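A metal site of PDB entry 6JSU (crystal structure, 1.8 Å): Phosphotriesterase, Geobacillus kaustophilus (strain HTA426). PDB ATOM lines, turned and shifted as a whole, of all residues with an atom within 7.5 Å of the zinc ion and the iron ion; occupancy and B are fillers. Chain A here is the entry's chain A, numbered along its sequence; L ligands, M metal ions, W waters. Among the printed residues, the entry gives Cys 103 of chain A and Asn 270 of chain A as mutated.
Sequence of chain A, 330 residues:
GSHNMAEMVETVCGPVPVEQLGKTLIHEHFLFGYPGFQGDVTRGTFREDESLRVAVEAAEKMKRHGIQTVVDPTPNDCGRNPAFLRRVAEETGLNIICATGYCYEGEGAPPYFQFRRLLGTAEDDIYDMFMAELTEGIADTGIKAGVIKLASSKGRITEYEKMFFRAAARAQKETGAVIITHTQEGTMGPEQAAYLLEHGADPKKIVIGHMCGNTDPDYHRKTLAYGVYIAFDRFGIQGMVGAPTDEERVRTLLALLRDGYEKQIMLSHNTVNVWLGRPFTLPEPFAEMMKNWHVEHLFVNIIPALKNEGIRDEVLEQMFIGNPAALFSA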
ATOM      1  N   HIS A  27     -22.559  -7.167  -7.602  1.00  0.00           N
ATOM      2  CA  HIS A  27     -21.616  -6.126  -7.146  1.00  0.00           C
ATOM      3  C   HIS A  27     -20.409  -6.057  -8.095  1.00  0.00           C
ATOM      4  O   HIS A  27     -19.426  -6.789  -7.930  1.00  0.00           O
ATOM      5  CB  HIS A  27     -21.185  -6.387  -5.685  1.00  0.00           C
ATOM      6  CG  HIS A  27     -20.585  -5.181  -4.995  1.00  0.00           C
ATOM      7  ND1 HIS A  27     -21.086  -4.704  -3.801  1.00  0.00           N
ATOM      8  CD2 HIS A  27     -19.579  -4.351  -5.349  1.00  0.00           C
ATOM      9  CE1 HIS A  27     -20.406  -3.634  -3.433  1.00  0.00           C
ATOM     10  NE2 HIS A  27     -19.475  -3.414  -4.341  1.00  0.00           N
ATOM     11  N   GLU A  28     -20.496  -5.170  -9.095  1.00  0.00           N
ATOM     12  CA  GLU A  28     -19.386  -4.862  -9.991  1.00  0.00           C
ATOM     13  C   GLU A  28     -19.388  -3.371 -10.311  1.00  0.00           C
ATOM     14  O   GLU A  28     -20.440  -2.741 -10.381  1.00  0.00           O
ATOM     15  CB  GLU A  28     -19.430  -5.673 -11.323  1.00  0.00           C
ATOM     16  CG  GLU A  28     -19.732  -7.144 -11.194  1.00  0.00           C
ATOM     17  CD  GLU A  28     -18.567  -7.975 -10.645  1.00  0.00           C
ATOM     18  OE1 GLU A  28     -17.409  -7.535 -10.769  1.00  0.00           O
ATOM     19  OE2 GLU A  28     -18.813  -9.081 -10.095  1.00  0.00           O
ATOM     20  N   HIS A  29     -18.194  -2.801 -10.489  1.00  0.00           N
ATOM     21  CA  HIS A  29     -18.047  -1.384 -10.833  1.00  0.00           C
ATOM     22  C   HIS A  29     -17.549  -1.234 -12.268  1.00  0.00           C
ATOM     23  O   HIS A  29     -16.449  -1.695 -12.598  1.00  0.00           O
ATOM     24  CB  HIS A  29     -17.088  -0.678  -9.869  1.00  0.00           C
ATOM     25  CG  HIS A  29     -17.485  -0.766  -8.429  1.00  0.00           C
ATOM     26  ND1 HIS A  29     -18.383   0.113  -7.853  1.00  0.00           N
ATOM     27  CD2 HIS A  29     -17.112  -1.625  -7.447  1.00  0.00           C
ATOM     28  CE1 HIS A  29     -18.546  -0.208  -6.581  1.00  0.00           C
ATOM     29  NE2 HIS A  29     -17.775  -1.247  -6.303  1.00  0.00           N
ATOM     30  N   PHE A  32     -14.861   3.525 -11.329  1.00  0.00           N
ATOM     31  CA  PHE A  32     -14.693   3.804  -9.906  1.00  0.00           C
ATOM     32  C   PHE A  32     -13.509   4.733  -9.729  1.00  0.00           C
ATOM     33  O   PHE A  32     -12.494   4.586 -10.411  1.00  0.00           O
ATOM     34  CB  PHE A  32     -14.457   2.524  -9.094  1.00  0.00           C
ATOM     35  CG  PHE A  32     -14.286   2.790  -7.610  1.00  0.00           C
ATOM     36  CD1 PHE A  32     -15.386   2.836  -6.768  1.00  0.00           C
ATOM     37  CD2 PHE A  32     -13.025   3.002  -7.066  1.00  0.00           C
ATOM     38  CE1 PHE A  32     -15.237   3.087  -5.417  1.00  0.00           C
ATOM     39  CE2 PHE A  32     -12.871   3.249  -5.727  1.00  0.00           C
ATOM     40  CZ  PHE A  32     -13.972   3.297  -4.902  1.00  0.00           C
ATOM     41  N   ASP A  72     -24.448  -2.154 -10.115  1.00  0.00           N
ATOM     42  CA  ASP A  72     -23.237  -1.353  -9.987  1.00  0.00           C
ATOM     43  C   ASP A  72     -23.448  -0.355  -8.850  1.00  0.00           C
ATOM     44  O   ASP A  72     -24.103   0.682  -9.038  1.00  0.00           O
ATOM     45  CB  ASP A  72     -22.925  -0.641 -11.307  1.00  0.00           C
ATOM     46  CG  ASP A  72     -21.646   0.167 -11.242  1.00  0.00           C
ATOM     47  OD1 ASP A  72     -21.306   0.664 -10.160  1.00  0.00           O
ATOM     48  OD2 ASP A  72     -20.965   0.321 -12.272  1.00  0.00           O
ATOM     49  N   PRO A  73     -22.920  -0.617  -7.670  1.00  0.00           N
ATOM     50  CA  PRO A  73     -23.254   0.233  -6.510  1.00  0.00           C
ATOM     51  C   PRO A  73     -22.211   1.312  -6.226  1.00  0.00           C
ATOM     52  O   PRO A  73     -22.011   1.686  -5.064  1.00  0.00           O
ATOM     53  CB  PRO A  73     -23.318  -0.779  -5.377  1.00  0.00           C
ATOM     54  CG  PRO A  73     -22.214  -1.747  -5.715  1.00  0.00           C
ATOM     55  CD  PRO A  73     -22.152  -1.802  -7.255  1.00  0.00           C
ATOM     56  N   THR A  74     -21.555   1.812  -7.273  1.00  0.00           N
ATOM     57  CA  THR A  74     -20.544   2.858  -7.112  1.00  0.00           C
ATOM     58  C   THR A  74     -21.097   4.048  -6.321  1.00  0.00           C
ATOM     59  O   THR A  74     -22.083   4.668  -6.746  1.00  0.00           O
ATOM     60  CB  THR A  74     -20.045   3.337  -8.475  1.00  0.00           C
ATOM     61  OG1 THR A  74     -19.491   2.218  -9.177  1.00  0.00           O
ATOM     62  CG2 THR A  74     -18.956   4.407  -8.305  1.00  0.00           C
ATOM     63  N   PRO A  75     -20.493   4.392  -5.180  1.00  0.00           N
ATOM     64  CA  PRO A  75     -21.045   5.457  -4.338  1.00  0.00           C
ATOM     65  C   PRO A  75     -21.003   6.827  -5.016  1.00  0.00           C
ATOM     66  O   PRO A  75     -20.219   7.074  -5.922  1.00  0.00           O
ATOM     67  CB  PRO A  75     -20.128   5.443  -3.104  1.00  0.00           C
ATOM     68  CG  PRO A  75     -19.650   4.018  -3.034  1.00  0.00           C
ATOM     69  CD  PRO A  75     -19.464   3.603  -4.478  1.00  0.00           C
ATOM     70  N   CYS A 103     -19.757   6.493   0.350  1.00  0.00           N
ATOM     71  CA  CYS A 103     -18.734   5.591   0.856  1.00  0.00           C
ATOM     72  C   CYS A 103     -18.615   5.683   2.386  1.00  0.00           C
ATOM     73  O   CYS A 103     -19.127   6.605   3.037  1.00  0.00           O
ATOM     74  CB  CYS A 103     -17.402   5.930   0.179  1.00  0.00           C
ATOM     75  SG  CYS A 103     -16.055   4.764   0.461  1.00  0.00           S
ATOM     76  N   TYR A 104     -17.885   4.728   2.971  1.00  0.00           N
ATOM     77  CA  TYR A 104     -17.658   4.793   4.403  1.00  0.00           C
ATOM     78  C   TYR A 104     -16.636   5.890   4.720  1.00  0.00           C
ATOM     79  O   TYR A 104     -15.884   6.355   3.855  1.00  0.00           O
ATOM     80  CB  TYR A 104     -17.182   3.448   4.976  1.00  0.00           C
ATOM     81  CG  TYR A 104     -15.822   2.977   4.510  1.00  0.00           C
ATOM     82  CD1 TYR A 104     -15.655   2.421   3.251  1.00  0.00           C
ATOM     83  CD2 TYR A 104     -14.716   3.081   5.340  1.00  0.00           C
ATOM     84  CE1 TYR A 104     -14.407   1.982   2.831  1.00  0.00           C
ATOM     85  CE2 TYR A 104     -13.480   2.644   4.938  1.00  0.00           C
ATOM     86  CZ  TYR A 104     -13.324   2.098   3.687  1.00  0.00           C
ATOM     87  OH  TYR A 104     -12.082   1.663   3.280  1.00  0.00           O
ATOM     88  N   KCX A 149     -26.957   2.349  -1.365  1.00  0.00           N
ATOM     89  CA  KCX A 149     -25.662   1.833  -0.959  1.00  0.00           C
ATOM     90  CB  KCX A 149     -24.595   2.183  -2.016  1.00  0.00           C
ATOM     91  CG  KCX A 149     -23.159   1.797  -1.618  1.00  0.00           C
ATOM     92  CD  KCX A 149     -23.043   0.283  -1.420  1.00  0.00           C
ATOM     93  CE  KCX A 149     -21.588  -0.141  -1.219  1.00  0.00           C
ATOM     94  NZ  KCX A 149     -20.820  -0.011  -2.502  1.00  0.00           N
ATOM     95  C   KCX A 149     -25.256   2.385   0.397  1.00  0.00           C
ATOM     96  O   KCX A 149     -25.281   3.587   0.609  1.00  0.00           O
ATOM     97  CX  KCX A 149     -19.623  -0.594  -2.613  1.00  0.00           C
ATOM     98  OQ1 KCX A 149     -19.184  -1.207  -1.623  1.00  0.00           O
ATOM     99  OQ2 KCX A 149     -18.949  -0.508  -3.655  1.00  0.00           O
ATOM    100  N   LEU A 150     -24.886   1.504   1.313  1.00  0.00           N
ATOM    101  CA  LEU A 150     -24.403   1.913   2.638  1.00  0.00           C
ATOM    102  C   LEU A 150     -23.032   1.305   2.890  1.00  0.00           C
ATOM    103  O   LEU A 150     -22.682   0.299   2.313  1.00  0.00           O
ATOM    104  CB  LEU A 150     -25.366   1.450   3.728  1.00  0.00           C
ATOM    105  CG  LEU A 150     -26.759   2.058   3.780  1.00  0.00           C
ATOM    106  CD1 LEU A 150     -27.553   1.302   4.841  1.00  0.00           C
ATOM    107  CD2 LEU A 150     -26.669   3.561   4.106  1.00  0.00           C
ATOM    108  N   ALA A 151     -22.261   1.897   3.798  1.00  0.00           N
ATOM    109  CA  ALA A 151     -20.911   1.393   4.063  1.00  0.00           C
ATOM    110  C   ALA A 151     -20.498   1.738   5.485  1.00  0.00           C
ATOM    111  O   ALA A 151     -20.832   2.818   5.987  1.00  0.00           O
ATOM    112  CB  ALA A 151     -19.905   1.986   3.075  1.00  0.00           C
ATOM    113  N   THR A 181     -24.850  -3.181   1.128  1.00  0.00           N
ATOM    114  CA  THR A 181     -23.843  -2.591   2.007  1.00  0.00           C
ATOM    115  C   THR A 181     -22.422  -3.035   1.661  1.00  0.00           C
ATOM    116  O   THR A 181     -22.205  -4.043   0.988  1.00  0.00           O
ATOM    117  CB  THR A 181     -24.097  -2.914   3.483  1.00  0.00           C
ATOM    118  OG1 THR A 181     -23.562  -4.208   3.806  1.00  0.00           O
ATOM    119  CG2 THR A 181     -25.579  -2.842   3.826  1.00  0.00           C
ATOM    120  N   HIS A 182     -21.488  -2.224   2.136  1.00  0.00           N
ATOM    121  CA  HIS A 182     -20.063  -2.504   2.178  1.00  0.00           C
ATOM    122  C   HIS A 182     -19.683  -2.737   3.639  1.00  0.00           C
ATOM    123  O   HIS A 182     -20.008  -1.914   4.500  1.00  0.00           O
ATOM    124  CB  HIS A 182     -19.308  -1.300   1.582  1.00  0.00           C
ATOM    125  CG  HIS A 182     -17.833  -1.289   1.835  1.00  0.00           C
ATOM    126  ND1 HIS A 182     -16.911  -1.342   0.808  1.00  0.00           N
ATOM    127  CD2 HIS A 182     -17.117  -1.111   2.974  1.00  0.00           C
ATOM    128  CE1 HIS A 182     -15.690  -1.273   1.312  1.00  0.00           C
ATOM    129  NE2 HIS A 182     -15.785  -1.134   2.623  1.00  0.00           N
ATOM    130  N   THR A 183     -19.007  -3.854   3.928  1.00  0.00           N
ATOM    131  CA  THR A 183     -18.329  -4.036   5.216  1.00  0.00           C
ATOM    132  C   THR A 183     -16.813  -3.961   4.989  1.00  0.00           C
ATOM    133  O   THR A 183     -16.312  -4.405   3.961  1.00  0.00           O
ATOM    134  CB  THR A 183     -18.665  -5.370   5.919  1.00  0.00           C
ATOM    135  OG1 THR A 183     -18.278  -6.507   5.105  1.00  0.00           O
ATOM    136  CG2 THR A 183     -20.159  -5.431   6.280  1.00  0.00           C
ATOM    137  N   GLN A 184     -16.106  -3.390   5.958  1.00  0.00           N
ATOM    138  CA  GLN A 184     -14.669  -3.192   5.865  1.00  0.00           C
ATOM    139  C   GLN A 184     -13.932  -4.302   6.628  1.00  0.00           C
ATOM    140  O   GLN A 184     -14.158  -4.508   7.834  1.00  0.00           O
ATOM    141  CB  GLN A 184     -14.307  -1.806   6.410  1.00  0.00           C
ATOM    142  CG  GLN A 184     -12.863  -1.393   6.221  1.00  0.00           C
ATOM    143  CD  GLN A 184     -12.452  -1.192   4.756  1.00  0.00           C
ATOM    144  OE1 GLN A 184     -13.281  -1.171   3.831  1.00  0.00           O
ATOM    145  NE2 GLN A 184     -11.149  -1.032   4.548  1.00  0.00           N
ATOM    146  N   GLY A 209     -22.738  -6.747   2.265  1.00  0.00           N
ATOM    147  CA  GLY A 209     -21.682  -7.025   1.299  1.00  0.00           C
ATOM    148  C   GLY A 209     -20.318  -7.306   1.927  1.00  0.00           C
ATOM    149  O   GLY A 209     -20.098  -7.094   3.112  1.00  0.00           O
ATOM    150  N   HIS A 210     -19.408  -7.779   1.063  1.00  0.00           N
ATOM    151  CA  HIS A 210     -18.033  -8.157   1.407  1.00  0.00           C
ATOM    152  C   HIS A 210     -17.949  -9.085   2.614  1.00  0.00           C
ATOM    153  O   HIS A 210     -17.010  -9.011   3.424  1.00  0.00           O
ATOM    154  CB  HIS A 210     -17.143  -6.919   1.637  1.00  0.00           C
ATOM    155  CG  HIS A 210     -17.316  -5.841   0.615  1.00  0.00           C
ATOM    156  ND1 HIS A 210     -17.596  -6.109  -0.705  1.00  0.00           N
ATOM    157  CD2 HIS A 210     -17.228  -4.490   0.711  1.00  0.00           C
ATOM    158  CE1 HIS A 210     -17.680  -4.969  -1.373  1.00  0.00           C
ATOM    159  NE2 HIS A 210     -17.470  -3.969  -0.535  1.00  0.00           N
ATOM    160  N   ASP A 233     -18.575 -11.203  -2.479  1.00  0.00           N
ATOM    161  CA  ASP A 233     -18.609 -10.358  -3.668  1.00  0.00           C
ATOM    162  C   ASP A 233     -17.240  -9.806  -4.023  1.00  0.00           C
ATOM    163  O   ASP A 233     -17.151  -8.864  -4.816  1.00  0.00           O
ATOM    164  CB  ASP A 233     -19.629  -9.223  -3.488  1.00  0.00           C
ATOM    165  CG  ASP A 233     -19.372  -8.402  -2.223  1.00  0.00           C
ATOM    166  OD1 ASP A 233     -18.238  -8.435  -1.728  1.00  0.00           O
ATOM    167  OD2 ASP A 233     -20.313  -7.717  -1.766  1.00  0.00           O
ATOM    168  N   ARG A 234     -16.157 -10.392  -3.497  1.00  0.00           N
ATOM    169  CA  ARG A 234     -14.807  -9.920  -3.801  1.00  0.00           C
ATOM    170  C   ARG A 234     -13.910 -11.047  -4.309  1.00  0.00           C
ATOM    171  O   ARG A 234     -12.696 -11.058  -4.085  1.00  0.00           O
ATOM    172  CB  ARG A 234     -14.177  -9.241  -2.572  1.00  0.00           C
ATOM    173  CG  ARG A 234     -14.743  -7.870  -2.315  1.00  0.00           C
ATOM    174  CD  ARG A 234     -14.052  -7.158  -1.128  1.00  0.00           C
ATOM    175  NE  ARG A 234     -14.026  -5.723  -1.344  1.00  0.00           N
ATOM    176  CZ  ARG A 234     -13.652  -4.844  -0.420  1.00  0.00           C
ATOM    177  NH1 ARG A 234     -13.273  -5.276   0.772  1.00  0.00           N
ATOM    178  NH2 ARG A 234     -13.665  -3.533  -0.698  1.00  0.00           N
ATOM    179  N   HIS A 269     -17.552 -10.182  -7.934  1.00  0.00           N
ATOM    180  CA  HIS A 269     -16.105  -9.911  -7.927  1.00  0.00           C
ATOM    181  C   HIS A 269     -15.725  -8.541  -7.386  1.00  0.00           C
ATOM    182  O   HIS A 269     -14.570  -8.352  -6.999  1.00  0.00           O
ATOM    183  CB  HIS A 269     -15.487  -9.963  -9.339  1.00  0.00           C
ATOM    184  CG  HIS A 269     -15.851 -11.169 -10.139  1.00  0.00           C
ATOM    185  ND1 HIS A 269     -16.979 -11.217 -10.933  1.00  0.00           N
ATOM    186  CD2 HIS A 269     -15.188 -12.334 -10.354  1.00  0.00           C
ATOM    187  CE1 HIS A 269     -17.015 -12.379 -11.579  1.00  0.00           C
ATOM    188  NE2 HIS A 269     -15.936 -13.070 -11.243  1.00  0.00           N
ATOM    189  N   ASN A 270     -16.645  -7.565  -7.415  1.00  0.00           N
ATOM    190  CA  ASN A 270     -16.330  -6.178  -7.076  1.00  0.00           C
ATOM    191  C   ASN A 270     -15.252  -5.614  -8.008  1.00  0.00           C
ATOM    192  O   ASN A 270     -14.394  -4.838  -7.577  1.00  0.00           O
ATOM    193  CB  ASN A 270     -15.918  -6.042  -5.598  1.00  0.00           C
ATOM    194  CG  ASN A 270     -15.860  -4.591  -5.124  1.00  0.00           C
ATOM    195  OD1 ASN A 270     -16.676  -3.755  -5.511  1.00  0.00           O
ATOM    196  ND2 ASN A 270     -14.878  -4.291  -4.260  1.00  0.00           N
ATOM    197  N   THR A 271     -15.284  -6.000  -9.288  1.00  0.00           N
ATOM    198  CA  THR A 271     -14.278  -5.476 -10.213  1.00  0.00           C
ATOM    199  C   THR A 271     -14.394  -3.964 -10.330  1.00  0.00           C
ATOM    200  O   THR A 271     -15.431  -3.350 -10.043  1.00  0.00           O
ATOM    201  CB  THR A 271     -14.405  -6.087 -11.624  1.00  0.00           C
ATOM    202  OG1 THR A 271     -15.736  -5.925 -12.109  1.00  0.00           O
ATOM    203  CG2 THR A 271     -14.008  -7.551 -11.639  1.00  0.00           C
ATOM    204  N   VAL A 272     -13.293  -3.352 -10.730  1.00  0.00           N
ATOM    205  CA  VAL A 272     -13.269  -1.965 -11.172  1.00  0.00           C
ATOM    206  C   VAL A 272     -12.715  -2.008 -12.590  1.00  0.00           C
ATOM    207  O   VAL A 272     -11.513  -2.241 -12.795  1.00  0.00           O
ATOM    208  CB  VAL A 272     -12.422  -1.071 -10.264  1.00  0.00           C
ATOM    209  CG1 VAL A 272     -12.207   0.285 -10.921  1.00  0.00           C
ATOM    210  CG2 VAL A 272     -13.103  -0.923  -8.879  1.00  0.00           C
HETATM  211  O1  LIG L   1     -16.429  -2.158  -2.949  1.00  0.00           O
HETATM  212 ZN    ZN M   1     -17.423  -1.971  -1.129  1.00  0.00          ZN
HETATM  213 FE    FE M   2     -17.822  -2.087  -4.514  1.00  0.00          FE
HETATM  214  O   HOH W   1     -16.598   0.648  -1.651  1.00  0.00           O
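Three residues have an atom within 4 Å of the zinc ion: KCX 149, His 182 and His 210.
The nearest printed residue that does not touch the zinc ion is His 27 (4.1 Å).
The backbone carbonyl oxygen (O) of Pro 73 is in hydrogen-bond range of NZ of KCX 149.
The side-chain carboxylate (OD1) of Asp 233 is in hydrogen-bond range of a ring nitrogen (ND1) of His 210 (2.6 Å).
The backbone NH (N) of Asn 270 is in hydrogen-bond range of the side-chain carboxylate (OE1) of Glu 28 (3.4 Å).
N of His 29 is in hydrogen-bond range of O of Thr 271 (2.9 Å).
N of Asn 270 sits at hydrogen-bond distance from O of Asp 233.
The backbone NH of His 182 sits at hydrogen-bond distance from the backbone carbonyl oxygen of Leu 150 (2.8 Å).
A ring nitrogen (ND1) of His 29 sits at hydrogen-bond distance from the side-chain hydroxyl of Thr 74, at 2.7 Å.
The backbone carbonyl oxygen of His 210 is in hydrogen-bond range of the side-chain hydroxyl of Thr 183, at 3.3 Å.
The zinc ion is bound by OQ1 of KCX 149 (2.0 Å).
The zinc ion is bound by O1 of the ligand, at 2.1 Å.
NE2 of His 210 binds the zinc ion, at 2.1 Å.
ND1 of His 182 is bound to the zinc ion, 2.1 Å away.
The zinc ion has four donor atoms within binding distance.
Slightly farther from the zinc ion lies water W1 (2.8 Å).
Of the 25 residues printed, 4 come within 4 Å of the iron ion.
The nearest printed residue that does not touch the iron ion is His 210 (4.3 Å).
The iron ion is bound by NE2 of His 29, at 2.0 Å.
O1 of the ligand binds the iron ion, 2.1 Å away.
OQ2 of KCX 149 is bound to the iron ion, 2.1 Å away.
A ring nitrogen (NE2) of His 27 is bound to the iron ion (2.1 Å).
The iron ion is bound by OD1 of Asn 270, 2.3 Å away.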
